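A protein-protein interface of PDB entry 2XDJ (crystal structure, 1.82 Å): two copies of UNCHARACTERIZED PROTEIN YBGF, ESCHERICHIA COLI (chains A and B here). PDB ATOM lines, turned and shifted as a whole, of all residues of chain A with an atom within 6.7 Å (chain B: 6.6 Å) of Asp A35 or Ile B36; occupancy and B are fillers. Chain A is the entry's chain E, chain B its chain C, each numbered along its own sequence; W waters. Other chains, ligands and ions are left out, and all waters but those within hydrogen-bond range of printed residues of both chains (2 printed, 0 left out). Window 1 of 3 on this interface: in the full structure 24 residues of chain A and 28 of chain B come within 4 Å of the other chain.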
ATOM      1  N   SER A  30      -7.566  -7.457  17.912  1.00  0.00           N
ATOM      2  CA  SER A  30      -8.628  -8.498  17.877  1.00  0.00           C
ATOM      3  C   SER A  30      -9.920  -7.994  17.299  1.00  0.00           C
ATOM      4  O   SER A  30     -10.605  -8.731  16.522  1.00  0.00           O
ATOM      5  CB  SER A  30      -8.962  -9.049  19.256  1.00  0.00           C
ATOM      6  OG  SER A  30      -7.828  -9.315  20.023  1.00  0.00           O
ATOM      7  N   ASP A  31     -10.296  -6.751  17.662  1.00  0.00           N
ATOM      8  CA  ASP A  31     -11.462  -6.145  17.059  1.00  0.00           C
ATOM      9  C   ASP A  31     -11.318  -6.037  15.533  1.00  0.00           C
ATOM     10  O   ASP A  31     -12.251  -6.363  14.791  1.00  0.00           O
ATOM     11  CB  ASP A  31     -11.743  -4.728  17.615  1.00  0.00           C
ATOM     12  CG  ASP A  31     -12.160  -4.705  19.077  1.00  0.00           C
ATOM     13  OD1 ASP A  31     -12.544  -5.741  19.652  1.00  0.00           O
ATOM     14  OD2 ASP A  31     -12.036  -3.599  19.669  1.00  0.00           O
ATOM     15  N   ASN A  32     -10.154  -5.577  15.060  1.00  0.00           N
ATOM     16  CA  ASN A  32      -9.927  -5.449  13.614  1.00  0.00           C
ATOM     17  C   ASN A  32      -9.917  -6.819  12.916  1.00  0.00           C
ATOM     18  O   ASN A  32     -10.448  -6.941  11.804  1.00  0.00           O
ATOM     19  CB  ASN A  32      -8.619  -4.718  13.290  1.00  0.00           C
ATOM     20  CG  ASN A  32      -8.630  -3.198  13.686  1.00  0.00           C
ATOM     21  OD1 ASN A  32      -9.695  -2.600  14.028  1.00  0.00           O
ATOM     22  ND2 ASN A  32      -7.426  -2.562  13.596  1.00  0.00           N
ATOM     23  N   GLN A  33      -9.402  -7.823  13.586  1.00  0.00           N
ATOM     24  CA  GLN A  33      -9.405  -9.177  13.027  1.00  0.00           C
ATOM     25  C   GLN A  33     -10.826  -9.708  12.895  1.00  0.00           C
ATOM     26  O   GLN A  33     -11.183 -10.217  11.864  1.00  0.00           O
ATOM     27  CB  GLN A  33      -8.585 -10.153  13.892  1.00  0.00           C
ATOM     28  CG  GLN A  33      -7.060  -9.870  14.008  1.00  0.00           C
ATOM     29  CD  GLN A  33      -6.360 -10.539  15.271  1.00  0.00           C
ATOM     30  OE1 GLN A  33      -6.896 -10.555  16.400  1.00  0.00           O
ATOM     31  NE2 GLN A  33      -5.155 -11.070  15.065  1.00  0.00           N
ATOM     32  N   SER A  34     -11.578  -9.629  13.989  1.00  0.00           N
ATOM     33  CA  SER A  34     -13.013  -9.979  14.005  1.00  0.00           C
ATOM     34  C   SER A  34     -13.840  -9.290  12.925  1.00  0.00           C
ATOM     35  O   SER A  34     -14.675  -9.947  12.258  1.00  0.00           O
ATOM     36  CB  SER A  34     -13.646  -9.802  15.396  1.00  0.00           C
ATOM     37  OG  SER A  34     -13.018 -10.732  16.253  1.00  0.00           O
ATOM     38  N   ASP A  35     -13.637  -8.000  12.737  1.00  0.00           N
ATOM     39  CA  ASP A  35     -14.290  -7.257  11.675  1.00  0.00           C
ATOM     40  C   ASP A  35     -13.922  -7.781  10.292  1.00  0.00           C
ATOM     41  O   ASP A  35     -14.827  -8.051   9.455  1.00  0.00           O
ATOM     42  CB  ASP A  35     -14.008  -5.759  11.795  1.00  0.00           C
ATOM     43  CG  ASP A  35     -14.811  -5.091  12.929  1.00  0.00           C
ATOM     44  OD1 ASP A  35     -15.989  -5.463  13.122  1.00  0.00           O
ATOM     45  OD2 ASP A  35     -14.273  -4.190  13.577  1.00  0.00           O
ATOM     46  N   ILE A  36     -12.614  -7.922  10.040  1.00  0.00           N
ATOM     47  CA  ILE A  36     -12.162  -8.560   8.786  1.00  0.00           C
ATOM     48  C   ILE A  36     -12.818  -9.925   8.517  1.00  0.00           C
ATOM     49  O   ILE A  36     -13.292 -10.177   7.383  1.00  0.00           O
ATOM     50  CB  ILE A  36     -10.650  -8.704   8.746  1.00  0.00           C
ATOM     51  CG1 ILE A  36     -10.064  -7.344   8.399  1.00  0.00           C
ATOM     52  CG2 ILE A  36     -10.216  -9.584   7.521  1.00  0.00           C
ATOM     53  CD1 ILE A  36     -10.640  -6.867   7.063  1.00  0.00           C
ATOM     54  N   ASP A  37     -12.836 -10.814   9.512  1.00  0.00           N
ATOM     55  CA  ASP A  37     -13.321 -12.170   9.256  1.00  0.00           C
ATOM     56  C   ASP A  37     -14.811 -12.172   8.986  1.00  0.00           C
ATOM     57  O   ASP A  37     -15.321 -12.901   8.099  1.00  0.00           O
ATOM     58  CB  ASP A  37     -12.965 -13.084  10.424  1.00  0.00           C
ATOM     59  CG  ASP A  37     -11.421 -13.232  10.616  1.00  0.00           C
ATOM     60  OD1 ASP A  37     -10.620 -12.884   9.678  1.00  0.00           O
ATOM     61  OD2 ASP A  37     -10.989 -13.656  11.720  1.00  0.00           O
ATOM     62  N   SER A  38     -15.530 -11.304   9.698  1.00  0.00           N
ATOM     63  CA  SER A  38     -16.956 -11.072   9.377  1.00  0.00           C
ATOM     64  C   SER A  38     -17.207 -10.517   7.941  1.00  0.00           C
ATOM     65  O   SER A  38     -18.053 -11.052   7.186  1.00  0.00           O
ATOM     66  CB  SER A  38     -17.626 -10.244  10.526  1.00  0.00           C
ATOM     67  OG  SER A  38     -18.844  -9.676  10.053  1.00  0.00           O
ATOM     68  N   LEU A  39     -16.460  -9.489   7.521  1.00  0.00           N
ATOM     69  CA  LEU A  39     -16.625  -8.936   6.183  1.00  0.00           C
ATOM     70  C   LEU A  39     -16.208  -9.957   5.088  1.00  0.00           C
ATOM     71  O   LEU A  39     -16.835  -9.982   4.036  1.00  0.00           O
ATOM     72  CB  LEU A  39     -15.809  -7.661   6.014  1.00  0.00           C
ATOM     73  CG  LEU A  39     -16.115  -6.518   7.001  1.00  0.00           C
ATOM     74  CD1 LEU A  39     -15.299  -5.294   6.611  1.00  0.00           C
ATOM     75  CD2 LEU A  39     -17.626  -6.213   6.952  1.00  0.00           C
ATOM     76  N   ARG A  40     -15.155 -10.727   5.321  1.00  0.00           N
ATOM     77  CA  ARG A  40     -14.798 -11.835   4.403  1.00  0.00           C
ATOM     78  C   ARG A  40     -15.997 -12.732   4.186  1.00  0.00           C
ATOM     79  O   ARG A  40     -16.408 -13.028   3.015  1.00  0.00           O
ATOM     80  CB  ARG A  40     -13.644 -12.673   4.955  1.00  0.00           C
ATOM     81  CG  ARG A  40     -12.300 -11.940   4.770  1.00  0.00           C
ATOM     82  CD  ARG A  40     -11.041 -12.813   5.041  1.00  0.00           C
ATOM     83  NE  ARG A  40     -11.011 -13.959   4.143  1.00  0.00           N
ATOM     84  CZ  ARG A  40     -10.141 -14.968   4.210  1.00  0.00           C
ATOM     85  NH1 ARG A  40     -10.219 -15.960   3.339  1.00  0.00           N
ATOM     86  NH2 ARG A  40      -9.221 -15.000   5.136  1.00  0.00           N
ATOM     87  N   LEU B  29      -3.154   0.851  14.184  1.00  0.00           N
ATOM     88  CA  LEU B  29      -4.392   0.137  14.571  1.00  0.00           C
ATOM     89  C   LEU B  29      -5.605   1.016  14.325  1.00  0.00           C
ATOM     90  O   LEU B  29      -6.642   0.569  13.788  1.00  0.00           O
ATOM     91  CB  LEU B  29      -4.274  -0.339  16.024  1.00  0.00           C
ATOM     92  CG  LEU B  29      -3.425  -1.647  16.185  1.00  0.00           C
ATOM     93  CD1 LEU B  29      -2.993  -1.849  17.617  1.00  0.00           C
ATOM     94  CD2 LEU B  29      -4.144  -2.913  15.704  1.00  0.00           C
ATOM     95  N   ASP B  31      -5.713   3.603  12.192  1.00  0.00           N
ATOM     96  CA  ASP B  31      -5.906   3.777  10.736  1.00  0.00           C
ATOM     97  C   ASP B  31      -6.547   2.529  10.164  1.00  0.00           C
ATOM     98  O   ASP B  31      -7.358   2.590   9.216  1.00  0.00           O
ATOM     99  CB  ASP B  31      -4.567   3.924  10.036  1.00  0.00           C
ATOM    100  CG  ASP B  31      -3.982   5.354  10.161  1.00  0.00           C
ATOM    101  OD1 ASP B  31      -4.677   6.233  10.685  1.00  0.00           O
ATOM    102  OD2 ASP B  31      -2.869   5.609   9.624  1.00  0.00           O
ATOM    103  N   ASN B  32      -6.189   1.376  10.698  1.00  0.00           N
ATOM    104  CA  ASN B  32      -6.732   0.147  10.095  1.00  0.00           C
ATOM    105  C   ASN B  32      -8.248  -0.029  10.391  1.00  0.00           C
ATOM    106  O   ASN B  32      -9.019  -0.436   9.558  1.00  0.00           O
ATOM    107  CB  ASN B  32      -5.968  -1.043  10.668  1.00  0.00           C
ATOM    108  CG  ASN B  32      -4.617  -1.225  10.020  1.00  0.00           C
ATOM    109  OD1 ASN B  32      -4.330  -0.710   8.911  1.00  0.00           O
ATOM    110  ND2 ASN B  32      -3.804  -1.984  10.664  1.00  0.00           N
ATOM    111  N   GLN B  33      -8.632   0.436  11.575  1.00  0.00           N
ATOM    112  CA  GLN B  33     -10.031   0.489  11.959  1.00  0.00           C
ATOM    113  C   GLN B  33     -10.784   1.393  10.953  1.00  0.00           C
ATOM    114  O   GLN B  33     -11.820   0.985  10.349  1.00  0.00           O
ATOM    115  CB  GLN B  33     -10.112   1.060  13.381  1.00  0.00           C
ATOM    116  CG  GLN B  33     -11.592   1.237  13.793  1.00  0.00           C
ATOM    117  CD  GLN B  33     -11.677   1.885  15.170  1.00  0.00           C
ATOM    118  OE1 GLN B  33     -11.147   2.950  15.342  1.00  0.00           O
ATOM    119  NE2 GLN B  33     -12.309   1.192  16.172  1.00  0.00           N
ATOM    120  N   SER B  34     -10.185   2.545  10.640  1.00  0.00           N
ATOM    121  CA  SER B  34     -10.758   3.399   9.550  1.00  0.00           C
ATOM    122  C   SER B  34     -10.793   2.748   8.161  1.00  0.00           C
ATOM    123  O   SER B  34     -11.784   2.867   7.428  1.00  0.00           O
ATOM    124  CB  SER B  34     -10.002   4.716   9.485  1.00  0.00           C
ATOM    125  OG  SER B  34     -10.187   5.395  10.739  1.00  0.00           O
ATOM    126  N   ASP B  35      -9.690   2.082   7.779  1.00  0.00           N
ATOM    127  CA  ASP B  35      -9.685   1.278   6.556  1.00  0.00           C
ATOM    128  C   ASP B  35     -10.835   0.276   6.442  1.00  0.00           C
ATOM    129  O   ASP B  35     -11.442   0.176   5.358  1.00  0.00           O
ATOM    130  CB  ASP B  35      -8.344   0.475   6.478  1.00  0.00           C
ATOM    131  CG  ASP B  35      -7.136   1.372   6.410  1.00  0.00           C
ATOM    132  OD1 ASP B  35      -7.295   2.563   5.986  1.00  0.00           O
ATOM    133  OD2 ASP B  35      -6.036   0.839   6.751  1.00  0.00           O
ATOM    134  N   ILE B  36     -11.055  -0.462   7.538  1.00  0.00           N
ATOM    135  CA  ILE B  36     -12.093  -1.457   7.634  1.00  0.00           C
ATOM    136  C   ILE B  36     -13.435  -0.784   7.504  1.00  0.00           C
ATOM    137  O   ILE B  36     -14.294  -1.315   6.863  1.00  0.00           O
ATOM    138  CB  ILE B  36     -11.961  -2.299   8.906  1.00  0.00           C
ATOM    139  CG1 ILE B  36     -10.651  -3.138   8.788  1.00  0.00           C
ATOM    140  CG2 ILE B  36     -13.245  -3.140   9.183  1.00  0.00           C
ATOM    141  CD1 ILE B  36     -10.185  -3.660  10.215  1.00  0.00           C
ATOM    142  N   ASP B  37     -13.609   0.406   8.113  1.00  0.00           N
ATOM    143  CA  ASP B  37     -14.907   1.097   7.915  1.00  0.00           C
ATOM    144  C   ASP B  37     -15.244   1.377   6.453  1.00  0.00           C
ATOM    145  O   ASP B  37     -16.395   1.195   6.005  1.00  0.00           O
ATOM    146  CB  ASP B  37     -14.899   2.407   8.700  1.00  0.00           C
ATOM    147  CG  ASP B  37     -14.889   2.218  10.161  1.00  0.00           C
ATOM    148  OD1 ASP B  37     -15.259   1.176  10.667  1.00  0.00           O
ATOM    149  OD2 ASP B  37     -14.421   3.159  10.870  1.00  0.00           O
ATOM    150  N   SER B  38     -14.213   1.745   5.675  1.00  0.00           N
ATOM    151  CA  SER B  38     -14.412   1.999   4.298  1.00  0.00           C
ATOM    152  C   SER B  38     -14.798   0.692   3.557  1.00  0.00           C
ATOM    153  O   SER B  38     -15.733   0.712   2.707  1.00  0.00           O
ATOM    154  CB  SER B  38     -13.191   2.704   3.653  1.00  0.00           C
ATOM    155  OG  SER B  38     -13.390   2.606   2.263  1.00  0.00           O
ATOM    156  N   LEU B  39     -14.146  -0.420   3.909  1.00  0.00           N
ATOM    157  CA  LEU B  39     -14.446  -1.717   3.268  1.00  0.00           C
ATOM    158  C   LEU B  39     -15.857  -2.189   3.584  1.00  0.00           C
ATOM    159  O   LEU B  39     -16.599  -2.681   2.717  1.00  0.00           O
ATOM    160  CB  LEU B  39     -13.408  -2.760   3.717  1.00  0.00           C
ATOM    161  CG  LEU B  39     -11.958  -2.413   3.341  1.00  0.00           C
ATOM    162  CD1 LEU B  39     -11.051  -3.667   3.622  1.00  0.00           C
ATOM    163  CD2 LEU B  39     -11.784  -1.936   1.971  1.00  0.00           C
ATOM    164  N   ARG B  40     -16.269  -1.946   4.828  1.00  0.00           N
ATOM    165  CA  ARG B  40     -17.597  -2.444   5.252  1.00  0.00           C
ATOM    166  C   ARG B  40     -18.640  -1.638   4.565  1.00  0.00           C
ATOM    167  O   ARG B  40     -19.693  -2.177   4.162  1.00  0.00           O
ATOM    168  CB  ARG B  40     -17.769  -2.305   6.755  1.00  0.00           C
ATOM    169  CG  ARG B  40     -19.216  -2.621   7.297  1.00  0.00           C
ATOM    170  CD  ARG B  40     -19.294  -2.353   8.795  1.00  0.00           C
ATOM    171  NE  ARG B  40     -18.264  -2.941   9.657  1.00  0.00           N
ATOM    172  CZ  ARG B  40     -17.210  -2.257  10.131  1.00  0.00           C
ATOM    173  NH1 ARG B  40     -16.991  -0.980   9.808  1.00  0.00           N
ATOM    174  NH2 ARG B  40     -16.328  -2.855  10.885  1.00  0.00           N
ATOM    175  N   GLY B  41     -18.363  -0.350   4.409  1.00  0.00           N
ATOM    176  CA  GLY B  41     -19.326   0.527   3.743  1.00  0.00           C
ATOM    177  C   GLY B  41     -19.500   0.081   2.307  1.00  0.00           C
ATOM    178  O   GLY B  41     -20.598   0.066   1.762  1.00  0.00           O
HETATM  179  O   HOH W   1     -17.757  -5.865  10.832  1.00  0.00           O
HETATM  180  O   HOH W   2      -5.070  -3.781  12.415  1.00  0.00           O
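Asn A32 touches its own counterpart, Asn B32. Asn A32 touches Gln B33, but with the chains exchanged Gln A33 does not touch Asn B32 (8.1 Å). Asn A32 touches Ile B36, but with the chains exchanged Ile A36 does not touch Asn B32 (7.1 Å). Leu A39 touches Arg B40, but with the chains exchanged Arg A40 does not touch Leu B39 (8.3 Å). Of the 8 pairs that touch across the chains among the printed residues, 1 has its exchanged pair printed and touching as well.
Hydrophobic or aromatic side chains of chain B within 4 Å of the printed part of chain A: Leu B29 and Ile B36. Hydrophobic or aromatic side chains of chain A within 4 Å of the printed part of chain B: Leu A39.
Among the printed residues, merely in contact across the chains: Asn A32 with Asn B32 (3.6 Å), Asn A32 with Ile B36 (3.6 Å), Asn A32 with Gln B33 (3.7 Å), Asp A35 with Ile B36 (3.8 Å), Leu A39 with Arg B40 (3.9 Å) and Leu A39 with Ile B36 (3.9 Å).
The side-chain carboxylate of Asp A35 lies within salt-bridge range of the guanidinium group of Arg B40 (3.5 Å). The backbone carbonyl oxygen (O) of Leu B29 is in hydrogen-bond range of the side-chain amide nitrogen (ND2) of Asn A32 (3.2 Å).
Water W2 bridges ND2 of Asn B32 (2.8 Å) and ND2 of Asn A32 (2.9 Å). Water W1 lies within hydrogen-bond range of the side-chain carboxylate of Asp A35 (2.9 Å) and the guanidinium group of Arg B40 (3.2 Å).
Of chain B, only Ile B36 and Arg B40 come within 4 Å of Asp A35. Of chain A, only Asn A32, Asp A35 and Leu A39 come within 4 Å of Ile B36. Of the printed residues of chain A, Gln B33 touches Asn A32 (3.7 Å). Of the printed residues of chain B, Leu A39 touches Ile B36 (3.9 Å) and Arg B40 (3.9 Å). Of the printed residues of chain A, Asn B32 touches Asn A32 (3.6 Å). Ser B34 touches none of the printed residues of chain A. Asp B37 touches none of the printed residues of chain A. The nearest residue of chain B that does not touch Asp A35 is Gln B33 (6.1 Å). The nearest residue of chain A that does not touch Ile B36 is Ile A36 (4.1 Å).
The side-chain amide oxygen (OD1) of Asn B32 lies close to the side-chain carboxylate (OD2) of Asp B35 (3.2 Å). NH1 of Arg B40 lies within salt-bridge range of OD1 of Asp B37.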
